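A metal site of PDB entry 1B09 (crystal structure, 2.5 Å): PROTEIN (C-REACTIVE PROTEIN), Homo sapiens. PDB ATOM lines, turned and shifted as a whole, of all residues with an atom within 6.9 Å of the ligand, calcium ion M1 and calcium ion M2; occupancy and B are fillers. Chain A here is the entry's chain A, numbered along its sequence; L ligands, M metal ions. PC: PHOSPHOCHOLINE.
The side-chain carboxylate of Glu 81 is in salt-bridge range of a nitrogen (N1) of the ligand (3.9 Å).
Merely in contact with calcium ion M2: Asp 60 (3.3 Å). The nearest printed residue that does not touch calcium ion M2 is Leu 64 (5.6 Å).
Calcium ion M1 is bound by an oxygen (O3) of the ligand (1.7 Å), the side-chain amide oxygen (OE1) of Gln 150 (2.5 Å), the side-chain carboxylate (OE1) of Glu 138 (2.5 Å), the side-chain carboxylate (OD2) of Asp 140 (2.5 Å), the side-chain carboxylate (OE2) of Glu 147 (2.8 Å) and the side-chain carboxylate (OD1) of Asp 140 (2.8 Å). Calcium ion M1 has six donor atoms within binding distance.
CD2 of Phe 66 touches C5 of the ligand, 3.5 Å away. Ser 74 touches the ligand (OG to C5, 3.5 Å). Hydrophobic or aromatic side chains within 4 Å of the ligand: Phe 66. Of the 22 residues printed, 8 come within 4 Å of the ligand. The nearest printed residue that does not touch the ligand is Gln 139 (4.002 Å).
The backbone carbonyl oxygen (O) of Asn 61 sits at hydrogen-bond distance from the backbone NH (N) of Gly 79 (3.2 Å). The backbone NH (N) of Asp 140 lies within hydrogen-bond range of the backbone carbonyl oxygen (O) of Asn 145 (3.3 Å). O of Ser 53 sits close to OE1 of Gln 139. The side-chain carboxylate (OD1) of Asp 60 sits close to the side-chain amide oxygen (OE1) of Gln 59, 3.4 Å away. OE1 of Gln 59 lies close to N of Asn 61 (3.2 Å). The backbone carbonyl oxygen of Phe 66 sits at hydrogen-bond distance from the backbone NH of Ser 74 (2.6 Å). OD1 of Asn 61 sits close to OD1 of Asp 60 (3.4 Å). The side-chain carboxylate of Glu 81 sits at hydrogen-bond distance from the side-chain hydroxyl of Ser 74, at 3.3 Å.
An oxygen (O1) of the ligand is bound to calcium ion M2. OD1 of Asn 61 binds calcium ion M2 (2.6 Å). Calcium ion M2 is bound by O of Gln 139, 2.7 Å away. OD1 of Asp 140 binds calcium ion M2 (2.7 Å). OE2 of Glu 138 is bound to calcium ion M2 (2.8 Å). Calcium ion M2 has five donor atoms within binding distance. Slightly farther from calcium ion M2 lies OE1 of Glu 138 (3.1 Å). Slightly farther from calcium ion M2 lies an oxygen (O4) of the ligand (3.1 Å).
The nearest printed residue that does not touch calcium ion M1 is Gln 139 (4.9 Å).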
ATOM      1  N   SER A  53     -31.428   0.434   9.145  1.00  0.00           N
ATOM      2  CA  SER A  53     -30.251  -0.342   9.575  1.00  0.00           C
ATOM      3  C   SER A  53     -30.202  -0.649  11.064  1.00  0.00           C
ATOM      4  O   SER A  53     -29.897   0.232  11.913  1.00  0.00           O
ATOM      5  CB  SER A  53     -28.995   0.441   9.162  1.00  0.00           C
ATOM      6  OG  SER A  53     -27.844  -0.381   9.383  1.00  0.00           O
ATOM      7  N   GLN A  59     -23.011  -8.246  15.331  1.00  0.00           N
ATOM      8  CA  GLN A  59     -23.526  -8.444  13.962  1.00  0.00           C
ATOM      9  C   GLN A  59     -24.064  -7.148  13.330  1.00  0.00           C
ATOM     10  O   GLN A  59     -25.141  -6.625  13.707  1.00  0.00           O
ATOM     11  CB  GLN A  59     -24.629  -9.503  14.054  1.00  0.00           C
ATOM     12  CG  GLN A  59     -25.514  -9.574  12.820  1.00  0.00           C
ATOM     13  CD  GLN A  59     -24.720 -10.150  11.674  1.00  0.00           C
ATOM     14  OE1 GLN A  59     -24.279  -9.465  10.767  1.00  0.00           O
ATOM     15  NE2 GLN A  59     -24.535 -11.482  11.747  1.00  0.00           N
ATOM     16  N   ASP A  60     -23.276  -6.600  12.365  1.00  0.00           N
ATOM     17  CA  ASP A  60     -23.612  -5.261  11.813  1.00  0.00           C
ATOM     18  C   ASP A  60     -24.828  -5.248  10.903  1.00  0.00           C
ATOM     19  O   ASP A  60     -25.319  -4.173  10.502  1.00  0.00           O
ATOM     20  CB  ASP A  60     -22.393  -4.745  11.037  1.00  0.00           C
ATOM     21  CG  ASP A  60     -22.111  -5.660   9.863  1.00  0.00           C
ATOM     22  OD1 ASP A  60     -22.921  -6.564   9.630  1.00  0.00           O
ATOM     23  OD2 ASP A  60     -21.107  -5.467   9.197  1.00  0.00           O
ATOM     24  N   ASN A  61     -25.296  -6.453  10.537  1.00  0.00           N
ATOM     25  CA  ASN A  61     -26.555  -6.537   9.825  1.00  0.00           C
ATOM     26  C   ASN A  61     -27.580  -7.389  10.550  1.00  0.00           C
ATOM     27  O   ASN A  61     -28.129  -8.350   9.972  1.00  0.00           O
ATOM     28  CB  ASN A  61     -26.266  -7.153   8.475  1.00  0.00           C
ATOM     29  CG  ASN A  61     -25.521  -6.172   7.621  1.00  0.00           C
ATOM     30  OD1 ASN A  61     -25.372  -5.007   7.945  1.00  0.00           O
ATOM     31  ND2 ASN A  61     -25.047  -6.697   6.476  1.00  0.00           N
ATOM     32  N   LEU A  64     -31.497  -5.579   8.233  1.00  0.00           N
ATOM     33  CA  LEU A  64     -31.253  -4.525   7.269  1.00  0.00           C
ATOM     34  C   LEU A  64     -32.244  -4.590   6.106  1.00  0.00           C
ATOM     35  O   LEU A  64     -32.529  -5.691   5.555  1.00  0.00           O
ATOM     36  CB  LEU A  64     -29.822  -4.710   6.723  1.00  0.00           C
ATOM     37  CG  LEU A  64     -29.392  -3.638   5.734  1.00  0.00           C
ATOM     38  CD1 LEU A  64     -28.913  -2.361   6.429  1.00  0.00           C
ATOM     39  CD2 LEU A  64     -28.207  -4.090   4.882  1.00  0.00           C
ATOM     40  N   PHE A  66     -32.634  -2.968   2.299  1.00  0.00           N
ATOM     41  CA  PHE A  66     -31.698  -2.324   1.373  1.00  0.00           C
ATOM     42  C   PHE A  66     -32.170  -2.390  -0.059  1.00  0.00           C
ATOM     43  O   PHE A  66     -32.750  -3.420  -0.514  1.00  0.00           O
ATOM     44  CB  PHE A  66     -30.372  -3.093   1.511  1.00  0.00           C
ATOM     45  CG  PHE A  66     -29.205  -2.273   0.980  1.00  0.00           C
ATOM     46  CD1 PHE A  66     -28.496  -1.451   1.847  1.00  0.00           C
ATOM     47  CD2 PHE A  66     -28.788  -2.420  -0.335  1.00  0.00           C
ATOM     48  CE1 PHE A  66     -27.363  -0.781   1.386  1.00  0.00           C
ATOM     49  CE2 PHE A  66     -27.662  -1.745  -0.785  1.00  0.00           C
ATOM     50  CZ  PHE A  66     -26.951  -0.920   0.071  1.00  0.00           C
ATOM     51  N   TRP A  67     -31.974  -1.282  -0.798  1.00  0.00           N
ATOM     52  CA  TRP A  67     -32.217  -1.340  -2.226  1.00  0.00           C
ATOM     53  C   TRP A  67     -30.938  -1.506  -3.015  1.00  0.00           C
ATOM     54  O   TRP A  67     -30.037  -0.618  -2.987  1.00  0.00           O
ATOM     55  CB  TRP A  67     -32.902  -0.042  -2.649  1.00  0.00           C
ATOM     56  CG  TRP A  67     -33.009  -0.001  -4.168  1.00  0.00           C
ATOM     57  CD1 TRP A  67     -32.094   0.613  -5.054  1.00  0.00           C
ATOM     58  CD2 TRP A  67     -34.088  -0.531  -5.004  1.00  0.00           C
ATOM     59  NE1 TRP A  67     -32.484   0.529  -6.354  1.00  0.00           N
ATOM     60  CE2 TRP A  67     -33.778  -0.192  -6.348  1.00  0.00           C
ATOM     61  CE3 TRP A  67     -35.266  -1.223  -4.740  1.00  0.00           C
ATOM     62  CZ2 TRP A  67     -34.625  -0.572  -7.377  1.00  0.00           C
ATOM     63  CZ3 TRP A  67     -36.119  -1.595  -5.769  1.00  0.00           C
ATOM     64  CH2 TRP A  67     -35.798  -1.261  -7.101  1.00  0.00           C
ATOM     65  N   SER A  68     -30.806  -2.668  -3.673  1.00  0.00           N
ATOM     66  CA  SER A  68     -29.694  -2.846  -4.621  1.00  0.00           C
ATOM     67  C   SER A  68     -30.108  -2.572  -6.047  1.00  0.00           C
ATOM     68  O   SER A  68     -31.053  -3.197  -6.600  1.00  0.00           O
ATOM     69  CB  SER A  68     -29.198  -4.278  -4.479  1.00  0.00           C
ATOM     70  OG  SER A  68     -30.321  -5.145  -4.268  1.00  0.00           O
ATOM     71  N   SER A  74     -33.520  -5.818  -0.993  1.00  0.00           N
ATOM     72  CA  SER A  74     -32.726  -6.808  -0.265  1.00  0.00           C
ATOM     73  C   SER A  74     -33.010  -6.781   1.221  1.00  0.00           C
ATOM     74  O   SER A  74     -32.988  -5.709   1.883  1.00  0.00           O
ATOM     75  CB  SER A  74     -31.260  -6.479  -0.522  1.00  0.00           C
ATOM     76  OG  SER A  74     -30.480  -6.889   0.607  1.00  0.00           O
ATOM     77  N   PHE A  75     -33.310  -7.990   1.783  1.00  0.00           N
ATOM     78  CA  PHE A  75     -33.739  -8.076   3.184  1.00  0.00           C
ATOM     79  C   PHE A  75     -32.944  -9.096   3.990  1.00  0.00           C
ATOM     80  O   PHE A  75     -32.996 -10.332   3.693  1.00  0.00           O
ATOM     81  CB  PHE A  75     -35.232  -8.469   3.175  1.00  0.00           C
ATOM     82  CG  PHE A  75     -35.758  -8.610   4.592  1.00  0.00           C
ATOM     83  CD1 PHE A  75     -35.684  -7.550   5.485  1.00  0.00           C
ATOM     84  CD2 PHE A  75     -36.341  -9.808   4.973  1.00  0.00           C
ATOM     85  CE1 PHE A  75     -36.204  -7.698   6.775  1.00  0.00           C
ATOM     86  CE2 PHE A  75     -36.853  -9.952   6.266  1.00  0.00           C
ATOM     87  CZ  PHE A  75     -36.788  -8.899   7.166  1.00  0.00           C
ATOM     88  N   THR A  76     -32.172  -8.604   4.967  1.00  0.00           N
ATOM     89  CA  THR A  76     -31.343  -9.538   5.739  1.00  0.00           C
ATOM     90  C   THR A  76     -31.538  -9.441   7.232  1.00  0.00           C
ATOM     91  O   THR A  76     -31.550  -8.339   7.840  1.00  0.00           O
ATOM     92  CB  THR A  76     -29.884  -9.267   5.402  1.00  0.00           C
ATOM     93  OG1 THR A  76     -29.114  -9.172   6.605  1.00  0.00           O
ATOM     94  CG2 THR A  76     -29.744  -7.972   4.602  1.00  0.00           C
ATOM     95  N   GLY A  79     -27.444 -11.406   9.382  1.00  0.00           N
ATOM     96  CA  GLY A  79     -26.317 -11.600   8.455  1.00  0.00           C
ATOM     97  C   GLY A  79     -26.697 -12.268   7.146  1.00  0.00           C
ATOM     98  O   GLY A  79     -25.924 -12.233   6.151  1.00  0.00           O
ATOM     99  N   GLU A  81     -29.022 -13.063   3.722  1.00  0.00           N
ATOM    100  CA  GLU A  81     -29.821 -12.274   2.792  1.00  0.00           C
ATOM    101  C   GLU A  81     -30.870 -13.071   2.053  1.00  0.00           C
ATOM    102  O   GLU A  81     -30.672 -14.295   1.733  1.00  0.00           O
ATOM    103  CB  GLU A  81     -28.848 -11.633   1.778  1.00  0.00           C
ATOM    104  CG  GLU A  81     -29.439 -10.423   1.038  1.00  0.00           C
ATOM    105  CD  GLU A  81     -28.345  -9.787   0.168  1.00  0.00           C
ATOM    106  OE1 GLU A  81     -27.178  -9.887   0.524  1.00  0.00           O
ATOM    107  OE2 GLU A  81     -28.680  -9.198  -0.862  1.00  0.00           O
ATOM    108  N   LEU A  83     -33.826 -12.055  -1.363  1.00  0.00           N
ATOM    109  CA  LEU A  83     -34.210 -10.977  -2.290  1.00  0.00           C
ATOM    110  C   LEU A  83     -35.686 -10.984  -2.673  1.00  0.00           C
ATOM    111  O   LEU A  83     -36.313 -12.048  -2.861  1.00  0.00           O
ATOM    112  CB  LEU A  83     -33.377 -11.116  -3.568  1.00  0.00           C
ATOM    113  CG  LEU A  83     -31.891 -10.917  -3.356  1.00  0.00           C
ATOM    114  CD1 LEU A  83     -31.056 -11.287  -4.588  1.00  0.00           C
ATOM    115  CD2 LEU A  83     -31.544  -9.463  -3.017  1.00  0.00           C
ATOM    116  N   GLU A 138     -25.634   3.446   6.460  1.00  0.00           N
ATOM    117  CA  GLU A 138     -25.490   2.020   6.722  1.00  0.00           C
ATOM    118  C   GLU A 138     -24.420   1.708   7.722  1.00  0.00           C
ATOM    119  O   GLU A 138     -23.254   2.229   7.634  1.00  0.00           O
ATOM    120  CB  GLU A 138     -25.184   1.305   5.393  1.00  0.00           C
ATOM    121  CG  GLU A 138     -25.741  -0.139   5.378  1.00  0.00           C
ATOM    122  CD  GLU A 138     -24.800  -1.070   6.146  1.00  0.00           C
ATOM    123  OE1 GLU A 138     -23.602  -0.933   6.020  1.00  0.00           O
ATOM    124  OE2 GLU A 138     -25.305  -1.937   6.873  1.00  0.00           O
ATOM    125  N   GLN A 139     -24.797   0.898   8.727  1.00  0.00           N
ATOM    126  CA  GLN A 139     -23.856   0.579   9.779  1.00  0.00           C
ATOM    127  C   GLN A 139     -22.954  -0.570   9.423  1.00  0.00           C
ATOM    128  O   GLN A 139     -23.424  -1.634   8.964  1.00  0.00           O
ATOM    129  CB  GLN A 139     -24.659   0.234  11.026  1.00  0.00           C
ATOM    130  CG  GLN A 139     -25.162   1.478  11.766  1.00  0.00           C
ATOM    131  CD  GLN A 139     -26.167   1.077  12.823  1.00  0.00           C
ATOM    132  OE1 GLN A 139     -27.174   0.441  12.570  1.00  0.00           O
ATOM    133  NE2 GLN A 139     -25.850   1.493  14.064  1.00  0.00           N
ATOM    134  N   ASP A 140     -21.632  -0.382   9.625  1.00  0.00           N
ATOM    135  CA  ASP A 140     -20.723  -1.523   9.612  1.00  0.00           C
ATOM    136  C   ASP A 140     -20.147  -1.804  10.989  1.00  0.00           C
ATOM    137  O   ASP A 140     -19.377  -2.783  11.196  1.00  0.00           O
ATOM    138  CB  ASP A 140     -19.598  -1.217   8.622  1.00  0.00           C
ATOM    139  CG  ASP A 140     -20.163  -1.276   7.223  1.00  0.00           C
ATOM    140  OD1 ASP A 140     -21.036  -2.103   6.995  1.00  0.00           O
ATOM    141  OD2 ASP A 140     -19.738  -0.488   6.382  1.00  0.00           O
ATOM    142  N   SER A 141     -20.472  -0.897  11.939  1.00  0.00           N
ATOM    143  CA  SER A 141     -20.235  -1.168  13.367  1.00  0.00           C
ATOM    144  C   SER A 141     -21.259  -0.466  14.236  1.00  0.00           C
ATOM    145  O   SER A 141     -22.031   0.415  13.781  1.00  0.00           O
ATOM    146  CB  SER A 141     -18.823  -0.682  13.720  1.00  0.00           C
ATOM    147  OG  SER A 141     -18.837   0.739  13.890  1.00  0.00           O
ATOM    148  N   ASN A 145     -19.125   3.635  11.324  1.00  0.00           N
ATOM    149  CA  ASN A 145     -18.554   3.126  10.068  1.00  0.00           C
ATOM    150  C   ASN A 145     -19.514   3.212   8.930  1.00  0.00           C
ATOM    151  O   ASN A 145     -20.020   2.191   8.400  1.00  0.00           O
ATOM    152  CB  ASN A 145     -18.108   1.687  10.313  1.00  0.00           C
ATOM    153  CG  ASN A 145     -16.814   1.701  11.110  1.00  0.00           C
ATOM    154  OD1 ASN A 145     -16.796   1.521  12.318  1.00  0.00           O
ATOM    155  ND2 ASN A 145     -15.715   1.939  10.383  1.00  0.00           N
ATOM    156  N   PHE A 146     -19.809   4.466   8.536  1.00  0.00           N
ATOM    157  CA  PHE A 146     -20.708   4.699   7.419  1.00  0.00           C
ATOM    158  C   PHE A 146     -19.998   4.774   6.081  1.00  0.00           C
ATOM    159  O   PHE A 146     -18.870   5.369   5.972  1.00  0.00           O
ATOM    160  CB  PHE A 146     -21.420   6.033   7.667  1.00  0.00           C
ATOM    161  CG  PHE A 146     -22.092   6.031   9.011  1.00  0.00           C
ATOM    162  CD1 PHE A 146     -22.668   4.874   9.499  1.00  0.00           C
ATOM    163  CD2 PHE A 146     -22.166   7.213   9.742  1.00  0.00           C
ATOM    164  CE1 PHE A 146     -23.327   4.894  10.715  1.00  0.00           C
ATOM    165  CE2 PHE A 146     -22.819   7.225  10.956  1.00  0.00           C
ATOM    166  CZ  PHE A 146     -23.398   6.065  11.454  1.00  0.00           C
ATOM    167  N   GLU A 147     -20.695   4.156   5.175  1.00  0.00           N
ATOM    168  CA  GLU A 147     -20.303   4.384   3.801  1.00  0.00           C
ATOM    169  C   GLU A 147     -21.168   5.464   3.142  1.00  0.00           C
ATOM    170  O   GLU A 147     -22.395   5.225   2.875  1.00  0.00           O
ATOM    171  CB  GLU A 147     -20.391   2.989   3.031  1.00  0.00           C
ATOM    172  CG  GLU A 147     -19.349   1.908   3.561  1.00  0.00           C
ATOM    173  CD  GLU A 147     -19.124   0.736   2.530  1.00  0.00           C
ATOM    174  OE1 GLU A 147     -18.754   1.022   1.399  1.00  0.00           O
ATOM    175  OE2 GLU A 147     -19.311  -0.416   2.911  1.00  0.00           O
ATOM    176  N   GLN A 150     -23.665   4.277   0.329  1.00  0.00           N
ATOM    177  CA  GLN A 150     -24.865   3.554   0.760  1.00  0.00           C
ATOM    178  C   GLN A 150     -25.881   4.508   1.336  1.00  0.00           C
ATOM    179  O   GLN A 150     -27.012   4.119   1.784  1.00  0.00           O
ATOM    180  CB  GLN A 150     -24.438   2.495   1.797  1.00  0.00           C
ATOM    181  CG  GLN A 150     -24.007   1.159   1.133  1.00  0.00           C
ATOM    182  CD  GLN A 150     -23.207   0.307   2.099  1.00  0.00           C
ATOM    183  OE1 GLN A 150     -22.311   0.741   2.794  1.00  0.00           O
ATOM    184  NE2 GLN A 150     -23.588  -0.998   2.109  1.00  0.00           N
HETATM  185  P1   PC L   1     -22.637  -3.835   4.296  1.00  0.00           P
HETATM  186  O1   PC L   1     -23.595  -3.692   5.536  1.00  0.00           O
HETATM  187  O3   PC L   1     -22.138  -2.396   4.339  1.00  0.00           O
HETATM  188  O4   PC L   1     -21.499  -4.685   4.846  1.00  0.00           O
HETATM  189  O2   PC L   1     -23.150  -4.166   2.819  1.00  0.00           O
HETATM  190  C1   PC L   1     -24.267  -5.065   2.536  1.00  0.00           C
HETATM  191  C2   PC L   1     -24.895  -5.148   1.084  1.00  0.00           C
HETATM  192  N1   PC L   1     -25.995  -6.135   0.708  1.00  0.00           N
HETATM  193  C3   PC L   1     -26.084  -7.144   1.773  1.00  0.00           C
HETATM  194  C4   PC L   1     -26.135  -6.770  -0.664  1.00  0.00           C
HETATM  195  C5   PC L   1     -27.268  -5.407   0.720  1.00  0.00           C
HETATM  196 CA    CA M   1     -21.515  -0.785   4.582  1.00  0.00          CA
HETATM  197 CA    CA M   2     -23.205  -3.737   7.290  1.00  0.00          CA
